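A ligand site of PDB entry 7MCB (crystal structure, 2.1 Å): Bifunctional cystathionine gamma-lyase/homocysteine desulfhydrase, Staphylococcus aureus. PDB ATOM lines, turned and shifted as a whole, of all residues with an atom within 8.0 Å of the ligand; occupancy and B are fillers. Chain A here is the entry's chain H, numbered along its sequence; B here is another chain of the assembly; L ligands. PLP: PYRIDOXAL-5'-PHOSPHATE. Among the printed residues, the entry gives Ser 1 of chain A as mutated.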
ATOM      1  N   SER A   1      -5.889 -18.885   7.232  1.00  0.00           N
ATOM      2  CA  SER A   1      -7.115 -19.089   6.471  1.00  0.00           C
ATOM      3  C   SER A   1      -8.138 -18.007   6.824  1.00  0.00           C
ATOM      4  O   SER A   1      -8.070 -16.902   6.289  1.00  0.00           O
ATOM      5  CB  SER A   1      -7.664 -20.488   6.728  1.00  0.00           C
ATOM      6  OG  SER A   1      -8.821 -20.748   5.944  1.00  0.00           O
ATOM      7  N   ASN A   2      -9.084 -18.301   7.718  1.00  0.00           N
ATOM      8  CA  ASN A   2     -10.095 -17.314   8.060  1.00  0.00           C
ATOM      9  C   ASN A   2      -9.541 -16.277   9.047  1.00  0.00           C
ATOM     10  O   ASN A   2      -8.473 -16.450   9.632  1.00  0.00           O
ATOM     11  CB  ASN A   2     -11.352 -17.997   8.606  1.00  0.00           C
ATOM     12  CG  ASN A   2     -12.100 -18.766   7.532  1.00  0.00           C
ATOM     13  OD1 ASN A   2     -12.129 -18.358   6.377  1.00  0.00           O
ATOM     14  ND2 ASN A   2     -12.725 -19.873   7.913  1.00  0.00           N
ATOM     15  N   LYS A   3     -10.296 -15.190   9.212  1.00  0.00           N
ATOM     16  CA  LYS A   3      -9.783 -14.004   9.918  1.00  0.00           C
ATOM     17  C   LYS A   3      -9.417 -14.292  11.373  1.00  0.00           C
ATOM     18  O   LYS A   3      -8.377 -13.840  11.854  1.00  0.00           O
ATOM     19  CB  LYS A   3     -10.828 -12.873   9.855  1.00  0.00           C
ATOM     20  CG  LYS A   3     -11.278 -12.512   8.453  1.00  0.00           C
ATOM     21  CD  LYS A   3     -11.958 -11.133   8.408  1.00  0.00           C
ATOM     22  CE  LYS A   3     -13.412 -11.204   8.924  1.00  0.00           C
ATOM     23  NZ  LYS A   3     -14.151  -9.913   8.754  1.00  0.00           N
ATOM     24  N   LYS A   4     -10.269 -15.032  12.086  1.00  0.00           N
ATOM     25  CA  LYS A   4      -9.973 -15.293  13.492  1.00  0.00           C
ATOM     26  C   LYS A   4      -8.728 -16.160  13.645  1.00  0.00           C
ATOM     27  O   LYS A   4      -8.015 -16.044  14.656  1.00  0.00           O
ATOM     28  CB  LYS A   4     -11.171 -15.946  14.162  1.00  0.00           C
ATOM     29  CG  LYS A   4     -12.327 -14.966  14.396  1.00  0.00           C
ATOM     30  CD  LYS A   4     -13.400 -15.603  15.268  1.00  0.00           C
ATOM     31  CE  LYS A   4     -14.750 -15.584  14.597  1.00  0.00           C
ATOM     32  NZ  LYS A   4     -15.832 -15.976  15.536  1.00  0.00           N
ATOM     33  N   THR A   5      -8.431 -17.009  12.656  1.00  0.00           N
ATOM     34  CA  THR A   5      -7.201 -17.800  12.714  1.00  0.00           C
ATOM     35  C   THR A   5      -5.986 -16.934  12.441  1.00  0.00           C
ATOM     36  O   THR A   5      -4.961 -17.051  13.109  1.00  0.00           O
ATOM     37  CB  THR A   5      -7.297 -18.943  11.702  1.00  0.00           C
ATOM     38  OG1 THR A   5      -8.464 -19.710  11.967  1.00  0.00           O
ATOM     39  CG2 THR A   5      -6.068 -19.856  11.776  1.00  0.00           C
ATOM     40  N   LYS A   6      -6.101 -16.032  11.460  1.00  0.00           N
ATOM     41  CA  LYS A   6      -5.004 -15.150  11.106  1.00  0.00           C
ATOM     42  C   LYS A   6      -4.618 -14.229  12.261  1.00  0.00           C
ATOM     43  O   LYS A   6      -3.440 -13.911  12.427  1.00  0.00           O
ATOM     44  CB  LYS A   6      -5.420 -14.352   9.858  1.00  0.00           C
ATOM     45  CG  LYS A   6      -4.355 -13.495   9.215  1.00  0.00           C
ATOM     46  CD  LYS A   6      -4.981 -12.803   7.997  1.00  0.00           C
ATOM     47  CE  LYS A   6      -4.021 -11.867   7.295  1.00  0.00           C
ATOM     48  NZ  LYS A   6      -4.707 -11.158   6.161  1.00  0.00           N
ATOM     49  N   LEU A   7      -5.603 -13.787  13.050  1.00  0.00           N
ATOM     50  CA  LEU A   7      -5.308 -12.986  14.231  1.00  0.00           C
ATOM     51  C   LEU A   7      -4.416 -13.716  15.217  1.00  0.00           C
ATOM     52  O   LEU A   7      -3.618 -13.086  15.919  1.00  0.00           O
ATOM     53  CB  LEU A   7      -6.606 -12.585  14.933  1.00  0.00           C
ATOM     54  CG  LEU A   7      -7.381 -11.479  14.234  1.00  0.00           C
ATOM     55  CD1 LEU A   7      -8.739 -11.383  14.888  1.00  0.00           C
ATOM     56  CD2 LEU A   7      -6.608 -10.179  14.358  1.00  0.00           C
ATOM     57  N   ILE A   8      -4.574 -15.027  15.327  1.00  0.00           N
ATOM     58  CA  ILE A   8      -3.800 -15.785  16.301  1.00  0.00           C
ATOM     59  C   ILE A   8      -2.431 -16.152  15.743  1.00  0.00           C
ATOM     60  O   ILE A   8      -1.416 -15.985  16.401  1.00  0.00           O
ATOM     61  CB  ILE A   8      -4.598 -17.027  16.743  1.00  0.00           C
ATOM     62  CG1 ILE A   8      -5.943 -16.593  17.316  1.00  0.00           C
ATOM     63  CG2 ILE A   8      -3.833 -17.828  17.802  1.00  0.00           C
ATOM     64  CD1 ILE A   8      -5.806 -15.472  18.366  1.00  0.00           C
ATOM     65  N   HIS A   9      -2.392 -16.596  14.487  1.00  0.00           N
ATOM     66  CA  HIS A   9      -1.169 -17.159  13.956  1.00  0.00           C
ATOM     67  C   HIS A   9      -0.446 -16.254  12.970  1.00  0.00           C
ATOM     68  O   HIS A   9       0.651 -16.607  12.529  1.00  0.00           O
ATOM     69  CB  HIS A   9      -1.481 -18.521  13.333  1.00  0.00           C
ATOM     70  CG  HIS A   9      -1.981 -19.504  14.332  1.00  0.00           C
ATOM     71  ND1 HIS A   9      -1.145 -20.115  15.249  1.00  0.00           N
ATOM     72  CD2 HIS A   9      -3.231 -19.946  14.609  1.00  0.00           C
ATOM     73  CE1 HIS A   9      -1.859 -20.917  16.026  1.00  0.00           C
ATOM     74  NE2 HIS A   9      -3.126 -20.826  15.655  1.00  0.00           N
ATOM     75  N   GLY A  10      -1.001 -15.094  12.636  1.00  0.00           N
ATOM     76  CA  GLY A  10      -0.338 -14.165  11.727  1.00  0.00           C
ATOM     77  C   GLY A  10       0.690 -13.282  12.423  1.00  0.00           C
ATOM     78  O   GLY A  10       0.519 -12.891  13.583  1.00  0.00           O
ATOM     79  N   GLY A  11       1.754 -12.942  11.705  1.00  0.00           N
ATOM     80  CA  GLY A  11       2.863 -12.216  12.275  1.00  0.00           C
ATOM     81  C   GLY A  11       3.796 -13.158  13.029  1.00  0.00           C
ATOM     82  O   GLY A  11       3.558 -14.353  13.151  1.00  0.00           O
ATOM     83  N   THR A  62       0.893  -7.968   8.515  1.00  0.00           N
ATOM     84  CA  THR A  62       0.163  -9.178   8.141  1.00  0.00           C
ATOM     85  C   THR A  62      -1.339  -8.935   8.096  1.00  0.00           C
ATOM     86  O   THR A  62      -2.027  -9.401   7.170  1.00  0.00           O
ATOM     87  CB  THR A  62       0.465 -10.303   9.153  1.00  0.00           C
ATOM     88  OG1 THR A  62       1.865 -10.585   9.163  1.00  0.00           O
ATOM     89  CG2 THR A  62      -0.293 -11.551   8.767  1.00  0.00           C
ATOM     90  N   LEU A  63      -1.879  -8.249   9.109  1.00  0.00           N
ATOM     91  CA  LEU A  63      -3.329  -8.075   9.199  1.00  0.00           C
ATOM     92  C   LEU A  63      -3.858  -7.144   8.108  1.00  0.00           C
ATOM     93  O   LEU A  63      -5.027  -7.279   7.700  1.00  0.00           O
ATOM     94  CB  LEU A  63      -3.706  -7.526  10.575  1.00  0.00           C
ATOM     95  CG  LEU A  63      -3.477  -8.476  11.763  1.00  0.00           C
ATOM     96  CD1 LEU A  63      -3.955  -7.813  13.032  1.00  0.00           C
ATOM     97  CD2 LEU A  63      -4.180  -9.802  11.561  1.00  0.00           C
ATOM     98  N   GLU A  64      -3.054  -6.191   7.656  1.00  0.00           N
ATOM     99  CA  GLU A  64      -3.448  -5.307   6.572  1.00  0.00           C
ATOM    100  C   GLU A  64      -2.946  -5.792   5.216  1.00  0.00           C
ATOM    101  O   GLU A  64      -3.084  -5.065   4.224  1.00  0.00           O
ATOM    102  CB  GLU A  64      -2.936  -3.889   6.838  1.00  0.00           C
ATOM    103  CG  GLU A  64      -3.615  -3.159   8.014  1.00  0.00           C
ATOM    104  CD  GLU A  64      -5.061  -2.698   7.723  1.00  0.00           C
ATOM    105  OE1 GLU A  64      -5.720  -3.242   6.820  1.00  0.00           O
ATOM    106  OE2 GLU A  64      -5.548  -1.794   8.447  1.00  0.00           O
ATOM    107  N   ASN A  65      -2.354  -6.987   5.154  1.00  0.00           N
ATOM    108  CA  ASN A  65      -1.868  -7.551   3.888  1.00  0.00           C
ATOM    109  C   ASN A  65      -0.835  -6.637   3.229  1.00  0.00           C
ATOM    110  O   ASN A  65      -0.806  -6.490   2.009  1.00  0.00           O
ATOM    111  CB  ASN A  65      -3.009  -7.839   2.903  1.00  0.00           C
ATOM    112  CG  ASN A  65      -3.969  -8.885   3.403  1.00  0.00           C
ATOM    113  OD1 ASN A  65      -3.578  -9.848   4.085  1.00  0.00           O
ATOM    114  ND2 ASN A  65      -5.255  -8.705   3.080  1.00  0.00           N
ATOM    115  N   ASN A 181      -9.681  -3.438   4.627  1.00  0.00           N
ATOM    116  CA  ASN A 181      -8.264  -3.551   4.294  1.00  0.00           C
ATOM    117  C   ASN A 181      -7.928  -2.607   3.138  1.00  0.00           C
ATOM    118  O   ASN A 181      -7.925  -3.017   1.972  1.00  0.00           O
ATOM    119  CB  ASN A 181      -7.897  -4.987   3.960  1.00  0.00           C
ATOM    120  CG  ASN A 181      -8.117  -5.931   5.141  1.00  0.00           C
ATOM    121  OD1 ASN A 181      -8.969  -6.823   5.102  1.00  0.00           O
ATOM    122  ND2 ASN A 181      -7.366  -5.702   6.216  1.00  0.00           N
ATOM    123  N   ASP A 184      -5.522  -3.553   0.204  1.00  0.00           N
ATOM    124  CA  ASP A 184      -6.082  -4.445  -0.807  1.00  0.00           C
ATOM    125  C   ASP A 184      -6.876  -3.696  -1.865  1.00  0.00           C
ATOM    126  O   ASP A 184      -7.133  -4.240  -2.934  1.00  0.00           O
ATOM    127  CB  ASP A 184      -7.016  -5.477  -0.174  1.00  0.00           C
ATOM    128  CG  ASP A 184      -6.265  -6.565   0.556  1.00  0.00           C
ATOM    129  OD1 ASP A 184      -5.030  -6.690   0.367  1.00  0.00           O
ATOM    130  OD2 ASP A 184      -6.915  -7.286   1.322  1.00  0.00           O
ATOM    131  N   SER B 316      -1.680 -27.736  11.092  1.00  0.00           N
ATOM    132  CA  SER B 316      -1.089 -26.405  10.985  1.00  0.00           C
ATOM    133  C   SER B 316      -1.448 -25.490  12.152  1.00  0.00           C
ATOM    134  O   SER B 316      -0.667 -24.576  12.467  1.00  0.00           O
ATOM    135  CB  SER B 316      -1.501 -25.722   9.676  1.00  0.00           C
ATOM    136  OG  SER B 316      -1.199 -26.534   8.553  1.00  0.00           O
ATOM    137  N   TYR B 317      -2.589 -25.707  12.803  1.00  0.00           N
ATOM    138  CA  TYR B 317      -3.103 -24.752  13.780  1.00  0.00           C
ATOM    139  C   TYR B 317      -3.156 -25.301  15.201  1.00  0.00           C
ATOM    140  O   TYR B 317      -3.691 -24.635  16.091  1.00  0.00           O
ATOM    141  CB  TYR B 317      -4.495 -24.255  13.344  1.00  0.00           C
ATOM    142  CG  TYR B 317      -4.512 -23.651  11.945  1.00  0.00           C
ATOM    143  CD1 TYR B 317      -3.610 -22.668  11.592  1.00  0.00           C
ATOM    144  CD2 TYR B 317      -5.421 -24.083  10.991  1.00  0.00           C
ATOM    145  CE1 TYR B 317      -3.603 -22.107  10.311  1.00  0.00           C
ATOM    146  CE2 TYR B 317      -5.428 -23.541   9.703  1.00  0.00           C
ATOM    147  CZ  TYR B 317      -4.523 -22.552   9.371  1.00  0.00           C
ATOM    148  OH  TYR B 317      -4.517 -22.004   8.103  1.00  0.00           O
ATOM    149  N   GLU B 364      -9.083 -19.696  17.467  1.00  0.00           N
ATOM    150  CA  GLU B 364      -9.045 -19.654  16.009  1.00  0.00           C
ATOM    151  C   GLU B 364     -10.436 -19.911  15.439  1.00  0.00           C
ATOM    152  O   GLU B 364     -11.341 -20.367  16.124  1.00  0.00           O
ATOM    153  CB  GLU B 364      -8.053 -20.685  15.461  1.00  0.00           C
ATOM    154  CG  GLU B 364      -6.631 -20.482  15.934  1.00  0.00           C
ATOM    155  CD  GLU B 364      -6.288 -21.374  17.136  1.00  0.00           C
ATOM    156  OE1 GLU B 364      -7.225 -21.753  17.869  1.00  0.00           O
ATOM    157  OE2 GLU B 364      -5.090 -21.686  17.327  1.00  0.00           O
ATOM    158  N   ASP B 368     -11.636 -23.589  10.452  1.00  0.00           N
ATOM    159  CA  ASP B 368     -10.221 -23.892  10.339  1.00  0.00           C
ATOM    160  C   ASP B 368      -9.792 -24.975  11.320  1.00  0.00           C
ATOM    161  O   ASP B 368      -9.059 -25.903  10.956  1.00  0.00           O
ATOM    162  CB  ASP B 368      -9.386 -22.634  10.555  1.00  0.00           C
ATOM    163  CG  ASP B 368      -9.449 -21.680   9.387  1.00  0.00           C
ATOM    164  OD1 ASP B 368      -9.816 -22.139   8.282  1.00  0.00           O
ATOM    165  OD2 ASP B 368      -9.150 -20.488   9.572  1.00  0.00           O
HETATM  166  N1  PLP L   1      -1.618 -15.950   7.880  1.00  0.00           N
HETATM  167  C2  PLP L   1      -2.206 -16.883   8.633  1.00  0.00           C
HETATM  168  C2A PLP L   1      -1.594 -17.265   9.956  1.00  0.00           C
HETATM  169  C3  PLP L   1      -3.395 -17.503   8.195  1.00  0.00           C
HETATM  170  O3  PLP L   1      -3.963 -18.462   8.981  1.00  0.00           O
HETATM  171  C4  PLP L   1      -3.974 -17.164   6.975  1.00  0.00           C
HETATM  172  C4A PLP L   1      -5.213 -17.833   6.539  1.00  0.00           C
HETATM  173  C5  PLP L   1      -3.315 -16.165   6.196  1.00  0.00           C
HETATM  174  C6  PLP L   1      -2.162 -15.604   6.699  1.00  0.00           C
HETATM  175  C5A PLP L   1      -3.843 -15.704   4.861  1.00  0.00           C
HETATM  176  O4P PLP L   1      -4.664 -14.548   5.049  1.00  0.00           O
HETATM  177  P   PLP L   1      -5.425 -13.852   3.808  1.00  0.00           P
HETATM  178  O1P PLP L   1      -4.484 -12.870   3.124  1.00  0.00           O
HETATM  179  O2P PLP L   1      -5.860 -14.926   2.851  1.00  0.00           O
HETATM  180  O3P PLP L   1      -6.625 -13.114   4.350  1.00  0.00           O
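C4A of the ligand is bonded to N of Ser 1, at 1.4 Å. The side-chain amino group (NZ) of Lys 6 is in salt-bridge range of an oxygen (O3P) of the ligand. The side-chain amide oxygen (OD1) of Asn 65 lies close to an oxygen (O1P) of the ligand, 3.3 Å away.
OD1 of Asp 368 of chain B sits at hydrogen-bond distance from OG of Ser 1 (2.9 Å). The side-chain amino group (NZ) of Lys 6 sits at hydrogen-bond distance from the side-chain amide oxygen (OD1) of Asn 65, at 2.7 Å. NZ of Lys 6 lies close to O of Thr 62 (3.4 Å). OD1 of Asn 65 lies close to O of Thr 62, 3.5 Å away. The side-chain amide nitrogen of Asn 65 lies within hydrogen-bond range of the side-chain carboxylate of Asp 184 (2.8 Å). The side-chain carboxylate (OE2) of Glu 364 of chain B is in hydrogen-bond range of a ring nitrogen (NE2) of His 9, 2.7 Å away. The side-chain carboxylate (OD2) of Asp 368 of chain B is in hydrogen-bond range of the side-chain hydroxyl (OG1) of Thr 5 (2.6 Å).
Merely in contact with the ligand: Thr 5, His 9, Gly 10 and Tyr 317 of chain B. Hydrophobic or aromatic side chains that line the ligand: His 9 and Tyr 317 of chain B. Of the 21 residues printed, 7 come within 4 Å of the ligand. The nearest printed residue that does not touch the ligand is Asn 2 (4.1 Å).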
